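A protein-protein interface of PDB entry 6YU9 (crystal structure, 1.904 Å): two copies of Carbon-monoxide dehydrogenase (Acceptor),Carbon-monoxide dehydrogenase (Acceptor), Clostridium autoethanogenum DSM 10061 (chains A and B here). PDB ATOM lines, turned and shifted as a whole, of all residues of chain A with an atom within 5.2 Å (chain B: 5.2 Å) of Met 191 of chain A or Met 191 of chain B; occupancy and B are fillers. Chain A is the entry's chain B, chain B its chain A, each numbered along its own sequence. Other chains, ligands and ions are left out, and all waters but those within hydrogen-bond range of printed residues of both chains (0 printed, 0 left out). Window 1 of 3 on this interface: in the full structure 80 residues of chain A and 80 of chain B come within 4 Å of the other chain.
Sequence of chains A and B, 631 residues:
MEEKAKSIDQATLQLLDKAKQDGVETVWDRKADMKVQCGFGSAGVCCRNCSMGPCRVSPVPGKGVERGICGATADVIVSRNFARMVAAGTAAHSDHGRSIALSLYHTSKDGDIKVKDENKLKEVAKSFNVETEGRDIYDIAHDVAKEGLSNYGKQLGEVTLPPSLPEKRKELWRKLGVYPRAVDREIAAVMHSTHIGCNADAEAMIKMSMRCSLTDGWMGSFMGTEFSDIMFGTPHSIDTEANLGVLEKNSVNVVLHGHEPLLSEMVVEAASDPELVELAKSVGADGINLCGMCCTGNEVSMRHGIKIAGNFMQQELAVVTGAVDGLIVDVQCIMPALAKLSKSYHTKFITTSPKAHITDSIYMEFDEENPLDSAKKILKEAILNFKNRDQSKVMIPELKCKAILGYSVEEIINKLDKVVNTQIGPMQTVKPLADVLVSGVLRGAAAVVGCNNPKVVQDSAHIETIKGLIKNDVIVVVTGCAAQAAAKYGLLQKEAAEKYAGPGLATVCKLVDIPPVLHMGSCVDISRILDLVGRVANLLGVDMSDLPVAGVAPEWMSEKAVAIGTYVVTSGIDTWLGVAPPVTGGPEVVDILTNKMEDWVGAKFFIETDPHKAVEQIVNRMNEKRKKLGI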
ATOM      1  N   ARG A  84      31.863 -22.028  10.481  1.00  0.00           N
ATOM      2  CA  ARG A  84      30.780 -22.142   9.482  1.00  0.00           C
ATOM      3  C   ARG A  84      29.512 -22.706  10.109  1.00  0.00           C
ATOM      4  O   ARG A  84      28.424 -22.325   9.687  1.00  0.00           O
ATOM      5  CB  ARG A  84      31.199 -22.988   8.270  1.00  0.00           C
ATOM      6  CG  ARG A  84      32.195 -22.220   7.404  1.00  0.00           C
ATOM      7  CD  ARG A  84      32.290 -22.726   5.985  1.00  0.00           C
ATOM      8  NE  ARG A  84      33.115 -21.827   5.173  1.00  0.00           N
ATOM      9  CZ  ARG A  84      33.415 -22.056   3.894  1.00  0.00           C
ATOM     10  NH1 ARG A  84      33.011 -23.172   3.298  1.00  0.00           N
ATOM     11  NH2 ARG A  84      34.160 -21.181   3.213  1.00  0.00           N
ATOM     12  N   ALA A  87      28.129 -19.524  11.622  1.00  0.00           N
ATOM     13  CA  ALA A  87      27.610 -18.648  10.591  1.00  0.00           C
ATOM     14  C   ALA A  87      26.255 -19.203  10.070  1.00  0.00           C
ATOM     15  O   ALA A  87      25.347 -18.430   9.751  1.00  0.00           O
ATOM     16  CB  ALA A  87      28.590 -18.575   9.437  1.00  0.00           C
ATOM     17  N   ALA A  88      26.142 -20.545   9.949  1.00  0.00           N
ATOM     18  CA  ALA A  88      24.932 -21.184   9.442  1.00  0.00           C
ATOM     19  C   ALA A  88      23.801 -21.070  10.446  1.00  0.00           C
ATOM     20  O   ALA A  88      22.674 -20.747  10.050  1.00  0.00           O
ATOM     21  CB  ALA A  88      25.201 -22.622   9.130  1.00  0.00           C
ATOM     22  N   ALA A  91      22.579 -17.596  10.426  1.00  0.00           N
ATOM     23  CA  ALA A  91      21.794 -17.301   9.229  1.00  0.00           C
ATOM     24  C   ALA A  91      20.344 -17.807   9.389  1.00  0.00           C
ATOM     25  O   ALA A  91      19.398 -17.098   9.006  1.00  0.00           O
ATOM     26  CB  ALA A  91      22.454 -17.885   7.980  1.00  0.00           C
ATOM     27  N   ILE A 187      27.895 -12.665   8.893  1.00  0.00           N
ATOM     28  CA  ILE A 187      27.788 -14.005   8.320  1.00  0.00           C
ATOM     29  C   ILE A 187      28.689 -14.047   7.059  1.00  0.00           C
ATOM     30  O   ILE A 187      29.388 -15.020   6.816  1.00  0.00           O
ATOM     31  CB  ILE A 187      26.298 -14.335   7.945  1.00  0.00           C
ATOM     32  CG1 ILE A 187      25.381 -14.500   9.198  1.00  0.00           C
ATOM     33  CG2 ILE A 187      26.223 -15.560   6.992  1.00  0.00           C
ATOM     34  CD1 ILE A 187      23.969 -14.315   8.936  1.00  0.00           C
ATOM     35  N   ALA A 188      28.694 -12.974   6.278  1.00  0.00           N
ATOM     36  CA  ALA A 188      29.558 -12.872   5.074  1.00  0.00           C
ATOM     37  C   ALA A 188      31.080 -12.818   5.511  1.00  0.00           C
ATOM     38  O   ALA A 188      31.942 -13.451   4.899  1.00  0.00           O
ATOM     39  CB  ALA A 188      29.200 -11.609   4.281  1.00  0.00           C
ATOM     40  N   ALA A 189      31.367 -12.146   6.630  1.00  0.00           N
ATOM     41  CA  ALA A 189      32.726 -12.064   7.138  1.00  0.00           C
ATOM     42  C   ALA A 189      33.274 -13.456   7.476  1.00  0.00           C
ATOM     43  O   ALA A 189      34.434 -13.746   7.157  1.00  0.00           O
ATOM     44  CB  ALA A 189      32.793 -11.159   8.386  1.00  0.00           C
ATOM     45  N   VAL A 190      32.488 -14.300   8.157  1.00  0.00           N
ATOM     46  CA  VAL A 190      32.964 -15.644   8.494  1.00  0.00           C
ATOM     47  C   VAL A 190      33.094 -16.514   7.221  1.00  0.00           C
ATOM     48  O   VAL A 190      34.052 -17.273   7.101  1.00  0.00           O
ATOM     49  CB  VAL A 190      32.028 -16.307   9.488  1.00  0.00           C
ATOM     50  CG1 VAL A 190      32.396 -17.776   9.652  1.00  0.00           C
ATOM     51  CG2 VAL A 190      32.029 -15.574  10.816  1.00  0.00           C
ATOM     52  N   MET A 191      32.121 -16.445   6.296  1.00  0.00           N
ATOM     53  CA  MET A 191      32.190 -17.240   5.075  1.00  0.00           C
ATOM     54  C   MET A 191      33.409 -16.833   4.239  1.00  0.00           C
ATOM     55  O   MET A 191      34.064 -17.691   3.654  1.00  0.00           O
ATOM     56  CB  MET A 191      30.916 -17.057   4.262  1.00  0.00           C
ATOM     57  CG  MET A 191      29.684 -17.634   4.913  1.00  0.00           C
ATOM     58  SD  MET A 191      29.855 -19.307   5.514  1.00  0.00           S
ATOM     59  CE  MET A 191      30.131 -20.126   3.944  1.00  0.00           C
ATOM     60  N   HIS A 192      33.745 -15.537   4.226  1.00  0.00           N
ATOM     61  CA  HIS A 192      34.916 -15.022   3.519  1.00  0.00           C
ATOM     62  C   HIS A 192      36.184 -15.540   4.190  1.00  0.00           C
ATOM     63  O   HIS A 192      37.023 -16.116   3.509  1.00  0.00           O
ATOM     64  CB  HIS A 192      34.973 -13.482   3.596  1.00  0.00           C
ATOM     65  CG  HIS A 192      36.220 -12.908   2.989  1.00  0.00           C
ATOM     66  ND1 HIS A 192      36.694 -11.662   3.347  1.00  0.00           N
ATOM     67  CD2 HIS A 192      37.058 -13.431   2.067  1.00  0.00           C
ATOM     68  CE1 HIS A 192      37.780 -11.463   2.637  1.00  0.00           C
ATOM     69  NE2 HIS A 192      38.014 -12.481   1.824  1.00  0.00           N
ATOM     70  N   SER A 193      36.347 -15.306   5.524  1.00  0.00           N
ATOM     71  CA  SER A 193      37.554 -15.707   6.241  1.00  0.00           C
ATOM     72  C   SER A 193      37.824 -17.209   6.289  1.00  0.00           C
ATOM     73  O   SER A 193      38.981 -17.583   6.521  1.00  0.00           O
ATOM     74  CB  SER A 193      37.548 -15.138   7.654  1.00  0.00           C
ATOM     75  OG  SER A 193      37.774 -13.740   7.572  1.00  0.00           O
ATOM     76  N   THR A 194      36.783 -18.074   6.105  1.00  0.00           N
ATOM     77  CA  THR A 194      36.981 -19.536   6.064  1.00  0.00           C
ATOM     78  C   THR A 194      37.296 -20.013   4.624  1.00  0.00           C
ATOM     79  O   THR A 194      37.601 -21.198   4.389  1.00  0.00           O
ATOM     80  CB  THR A 194      35.781 -20.230   6.666  1.00  0.00           C
ATOM     81  OG1 THR A 194      34.641 -19.952   5.882  1.00  0.00           O
ATOM     82  CG2 THR A 194      35.524 -19.805   8.149  1.00  0.00           C
ATOM     83  N   HIS A 195      37.267 -19.088   3.653  1.00  0.00           N
ATOM     84  CA  HIS A 195      37.572 -19.435   2.255  1.00  0.00           C
ATOM     85  C   HIS A 195      39.048 -19.849   2.204  1.00  0.00           C
ATOM     86  O   HIS A 195      39.840 -19.297   2.969  1.00  0.00           O
ATOM     87  CB  HIS A 195      37.312 -18.204   1.366  1.00  0.00           C
ATOM     88  CG  HIS A 195      37.545 -18.414  -0.116  1.00  0.00           C
ATOM     89  ND1 HIS A 195      38.832 -18.521  -0.650  1.00  0.00           N
ATOM     90  CD2 HIS A 195      36.654 -18.507  -1.140  1.00  0.00           C
ATOM     91  CE1 HIS A 195      38.673 -18.710  -1.964  1.00  0.00           C
ATOM     92  NE2 HIS A 195      37.390 -18.647  -2.312  1.00  0.00           N
ATOM     93  N   ARG B  84      26.742 -24.026  -0.653  1.00  0.00           N
ATOM     94  CA  ARG B  84      27.641 -23.357   0.291  1.00  0.00           C
ATOM     95  C   ARG B  84      28.952 -22.923  -0.407  1.00  0.00           C
ATOM     96  O   ARG B  84      29.556 -21.915  -0.012  1.00  0.00           O
ATOM     97  CB  ARG B  84      27.883 -24.225   1.518  1.00  0.00           C
ATOM     98  CG  ARG B  84      26.658 -24.288   2.388  1.00  0.00           C
ATOM     99  CD  ARG B  84      26.903 -24.813   3.796  1.00  0.00           C
ATOM    100  NE  ARG B  84      25.671 -24.715   4.595  1.00  0.00           N
ATOM    101  CZ  ARG B  84      25.551 -25.085   5.878  1.00  0.00           C
ATOM    102  NH1 ARG B  84      26.572 -25.641   6.534  1.00  0.00           N
ATOM    103  NH2 ARG B  84      24.385 -24.911   6.512  1.00  0.00           N
ATOM    104  N   ALA B  87      27.901 -19.666  -1.921  1.00  0.00           N
ATOM    105  CA  ALA B  87      27.734 -18.646  -0.891  1.00  0.00           C
ATOM    106  C   ALA B  87      29.091 -18.152  -0.406  1.00  0.00           C
ATOM    107  O   ALA B  87      29.280 -16.946  -0.205  1.00  0.00           O
ATOM    108  CB  ALA B  87      26.929 -19.205   0.292  1.00  0.00           C
ATOM    109  N   ALA B  88      30.043 -19.087  -0.169  1.00  0.00           N
ATOM    110  CA  ALA B  88      31.389 -18.764   0.333  1.00  0.00           C
ATOM    111  C   ALA B  88      32.186 -17.946  -0.688  1.00  0.00           C
ATOM    112  O   ALA B  88      32.884 -17.025  -0.290  1.00  0.00           O
ATOM    113  CB  ALA B  88      32.128 -20.041   0.646  1.00  0.00           C
ATOM    114  N   ALA B  91      30.760 -14.556  -0.750  1.00  0.00           N
ATOM    115  CA  ALA B  91      31.200 -13.806   0.437  1.00  0.00           C
ATOM    116  C   ALA B  91      32.640 -13.265   0.247  1.00  0.00           C
ATOM    117  O   ALA B  91      32.928 -12.166   0.683  1.00  0.00           O
ATOM    118  CB  ALA B  91      31.121 -14.661   1.670  1.00  0.00           C
ATOM    119  N   GLU B 186      21.563 -12.441   0.273  1.00  0.00           N
ATOM    120  CA  GLU B 186      21.505 -13.694  -0.484  1.00  0.00           C
ATOM    121  C   GLU B 186      22.454 -14.734   0.134  1.00  0.00           C
ATOM    122  O   GLU B 186      22.160 -15.938   0.108  1.00  0.00           O
ATOM    123  CB  GLU B 186      21.949 -13.520  -1.955  1.00  0.00           C
ATOM    124  CG  GLU B 186      21.012 -12.780  -2.884  1.00  0.00           C
ATOM    125  CD  GLU B 186      19.610 -13.311  -3.024  1.00  0.00           C
ATOM    126  OE1 GLU B 186      19.316 -14.439  -2.561  1.00  0.00           O
ATOM    127  OE2 GLU B 186      18.799 -12.591  -3.645  1.00  0.00           O
ATOM    128  N   ILE B 187      23.621 -14.287   0.636  1.00  0.00           N
ATOM    129  CA  ILE B 187      24.559 -15.228   1.263  1.00  0.00           C
ATOM    130  C   ILE B 187      23.858 -15.829   2.486  1.00  0.00           C
ATOM    131  O   ILE B 187      23.819 -17.048   2.614  1.00  0.00           O
ATOM    132  CB  ILE B 187      25.900 -14.520   1.664  1.00  0.00           C
ATOM    133  CG1 ILE B 187      26.731 -14.096   0.400  1.00  0.00           C
ATOM    134  CG2 ILE B 187      26.749 -15.374   2.635  1.00  0.00           C
ATOM    135  CD1 ILE B 187      27.748 -12.897   0.685  1.00  0.00           C
ATOM    136  N   ALA B 188      23.194 -14.992   3.300  1.00  0.00           N
ATOM    137  CA  ALA B 188      22.477 -15.503   4.482  1.00  0.00           C
ATOM    138  C   ALA B 188      21.317 -16.441   4.062  1.00  0.00           C
ATOM    139  O   ALA B 188      21.028 -17.406   4.758  1.00  0.00           O
ATOM    140  CB  ALA B 188      21.924 -14.368   5.292  1.00  0.00           C
ATOM    141  N   ALA B 189      20.614 -16.122   2.968  1.00  0.00           N
ATOM    142  CA  ALA B 189      19.503 -16.969   2.484  1.00  0.00           C
ATOM    143  C   ALA B 189      19.978 -18.386   2.185  1.00  0.00           C
ATOM    144  O   ALA B 189      19.271 -19.347   2.520  1.00  0.00           O
ATOM    145  CB  ALA B 189      18.883 -16.371   1.220  1.00  0.00           C
ATOM    146  N   VAL B 190      21.152 -18.524   1.507  1.00  0.00           N
ATOM    147  CA  VAL B 190      21.688 -19.853   1.168  1.00  0.00           C
ATOM    148  C   VAL B 190      22.145 -20.573   2.437  1.00  0.00           C
ATOM    149  O   VAL B 190      21.871 -21.750   2.580  1.00  0.00           O
ATOM    150  CB  VAL B 190      22.851 -19.768   0.149  1.00  0.00           C
ATOM    151  CG1 VAL B 190      23.546 -21.122   0.010  1.00  0.00           C
ATOM    152  CG2 VAL B 190      22.356 -19.277  -1.216  1.00  0.00           C
ATOM    153  N   MET B 191      22.826 -19.868   3.358  1.00  0.00           N
ATOM    154  CA  MET B 191      23.288 -20.496   4.574  1.00  0.00           C
ATOM    155  C   MET B 191      22.078 -21.000   5.411  1.00  0.00           C
ATOM    156  O   MET B 191      22.141 -22.103   5.987  1.00  0.00           O
ATOM    157  CB  MET B 191      24.162 -19.513   5.363  1.00  0.00           C
ATOM    158  CG  MET B 191      25.533 -19.224   4.698  1.00  0.00           C
ATOM    159  SD  MET B 191      26.491 -20.745   4.210  1.00  0.00           S
ATOM    160  CE  MET B 191      26.765 -21.431   5.815  1.00  0.00           C
ATOM    161  N   HIS B 192      20.960 -20.235   5.404  1.00  0.00           N
ATOM    162  CA  HIS B 192      19.734 -20.644   6.080  1.00  0.00           C
ATOM    163  C   HIS B 192      19.136 -21.891   5.435  1.00  0.00           C
ATOM    164  O   HIS B 192      18.924 -22.907   6.103  1.00  0.00           O
ATOM    165  CB  HIS B 192      18.688 -19.531   6.052  1.00  0.00           C
ATOM    166  CG  HIS B 192      17.343 -19.954   6.587  1.00  0.00           C
ATOM    167  ND1 HIS B 192      16.175 -19.292   6.228  1.00  0.00           N
ATOM    168  CD2 HIS B 192      17.013 -20.969   7.422  1.00  0.00           C
ATOM    169  CE1 HIS B 192      15.192 -19.912   6.863  1.00  0.00           C
ATOM    170  NE2 HIS B 192      15.645 -20.925   7.586  1.00  0.00           N
ATOM    171  N   SER B 193      18.873 -21.828   4.136  1.00  0.00           N
ATOM    172  CA  SER B 193      18.254 -22.941   3.436  1.00  0.00           C
ATOM    173  C   SER B 193      19.069 -24.234   3.418  1.00  0.00           C
ATOM    174  O   SER B 193      18.493 -25.283   3.132  1.00  0.00           O
ATOM    175  CB  SER B 193      17.904 -22.518   2.022  1.00  0.00           C
ATOM    176  OG  SER B 193      16.864 -21.557   2.104  1.00  0.00           O
ATOM    177  N   THR B 194      20.392 -24.178   3.650  1.00  0.00           N
ATOM    178  CA  THR B 194      21.196 -25.405   3.661  1.00  0.00           C
ATOM    179  C   THR B 194      21.258 -25.966   5.098  1.00  0.00           C
ATOM    180  O   THR B 194      21.766 -27.064   5.303  1.00  0.00           O
ATOM    181  CB  THR B 194      22.584 -25.144   3.060  1.00  0.00           C
ATOM    182  OG1 THR B 194      23.272 -24.159   3.846  1.00  0.00           O
ATOM    183  CG2 THR B 194      22.521 -24.710   1.592  1.00  0.00           C
ATOM    184  N   HIS B 195      20.691 -25.247   6.085  1.00  0.00           N
ATOM    185  CA  HIS B 195      20.638 -25.718   7.448  1.00  0.00           C
ATOM    186  C   HIS B 195      19.763 -27.010   7.504  1.00  0.00           C
ATOM    187  O   HIS B 195      18.955 -27.274   6.585  1.00  0.00           O
ATOM    188  CB  HIS B 195      20.059 -24.617   8.343  1.00  0.00           C
ATOM    189  CG  HIS B 195      20.061 -24.933   9.798  1.00  0.00           C
ATOM    190  ND1 HIS B 195      19.097 -25.769  10.360  1.00  0.00           N
ATOM    191  CD2 HIS B 195      20.807 -24.405  10.802  1.00  0.00           C
ATOM    192  CE1 HIS B 195      19.353 -25.792  11.663  1.00  0.00           C
ATOM    193  NE2 HIS B 195      20.401 -25.025  11.968  1.00  0.00           N
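The guanidinium group of Arg 84 of chain B sits at hydrogen-bond distance from the side-chain hydroxyl of Thr 194 of chain B (2.6 Å). The backbone carbonyl oxygen (O) of Met 191 of chain B is in hydrogen-bond range of the side-chain hydroxyl (OG1) of Thr 194 of chain B, 3.2 Å away. The side-chain hydroxyl (OG1) of Thr 194 of chain A sits at hydrogen-bond distance from the backbone carbonyl oxygen (O) of Met 191 of chain A, 3.2 Å away. The guanidinium group of Arg 84 of chain A is in hydrogen-bond range of the side-chain hydroxyl of Thr 194 of chain A.
Among the printed residues, pairs that only touch across the chains: Arg 84 of chain A with Ala 88 of chain B (3.5 Å), Ala 88 of chain A with Arg 84 of chain B (3.6 Å), Ala 88 of chain A with Met 191 of chain B (3.9 Å), Ala 91 of chain A with Ala 188 of chain B (3.6 Å), Ala 91 of chain A with Met 191 of chain B (3.5 Å), Ala 91 of chain A with His 192 of chain B (3.8 Å), Ala 188 of chain A with Ala 91 of chain B (3.5 Å), Met 191 of chain A with Ala 88 of chain B (3.9 Å), Met 191 of chain A with Ala 91 of chain B (3.5 Å), Met 191 of chain A with Met 191 of chain B (3.7 Å) and His 192 of chain A with Ala 91 of chain B (3.8 Å).
Ala 87 of chain A touches none of the printed residues of chain B. Of the printed residues of chain B, Ala 88 of chain A touches Arg 84 (3.6 Å) and Met 191 (3.9 Å). Printed residues of chain B within 4 Å of Ala 188 of chain A: Ala 91 (3.5 Å). Met 191 of chain A touches three residues of chain B. Of the printed residues of chain B, His 192 of chain A touches Ala 91. Of the printed residues of chain A, Arg 84 of chain B touches Ala 88. Of the printed residues of chain A, Met 191 of chain B touches Ala 88 (3.9 Å), Ala 91 (3.5 Å) and Met 191 (3.7 Å). Printed residues of chain A within 4 Å of His 192 of chain B: Ala 91 (3.8 Å). The nearest residue of chain B that does not touch Met 191 of chain A is Ile 187 of chain B (4.3 Å). The nearest residue of chain A that does not touch Met 191 of chain B is Arg 84 of chain A (4.3 Å).
Of the 14 printed residues of chain B, 6 touch a printed residue of chain A. Printed residues of chain B that touch a printed residue of chain A: Arg 84, Ala 88, Ala 91, Ala 188, Met 191 and His 192. Hydrophobic or aromatic side chains of chain B within 4 Å of the printed part of chain A: Ala 88, Ala 91, Met 191 and His 192. Of the 13 printed residues of chain A, 6 touch a printed residue of chain B. Hydrophobic or aromatic side chains of chain A that line the printed part of chain B: Ala 88, Ala 91, Met 191 and His 192. Among the printed residues, 11 pairs touch across the chains. Among the printed residues, no Asp or Glu carboxylate lies within 4 Å of a Lys or Arg side-chain nitrogen of the other chain.
Ala 88 of chain A touches Met 191 of chain B, and with the chains exchanged Met 191 of chain A touches Ala 88 of chain B. Ala 91 of chain A touches Met 191 of chain B, and with the chains exchanged Met 191 of chain A touches Ala 91 of chain B. Ala 91 of chain A touches His 192 of chain B, and with the chains exchanged His 192 of chain A touches Ala 91 of chain B. Met 191 of chain A touches its own counterpart, Met 191 of chain B. 13 positions are printed for both chains. Of the 11 pairs that touch across the chains among the printed residues, 11 have their exchanged pair printed and touching as well.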
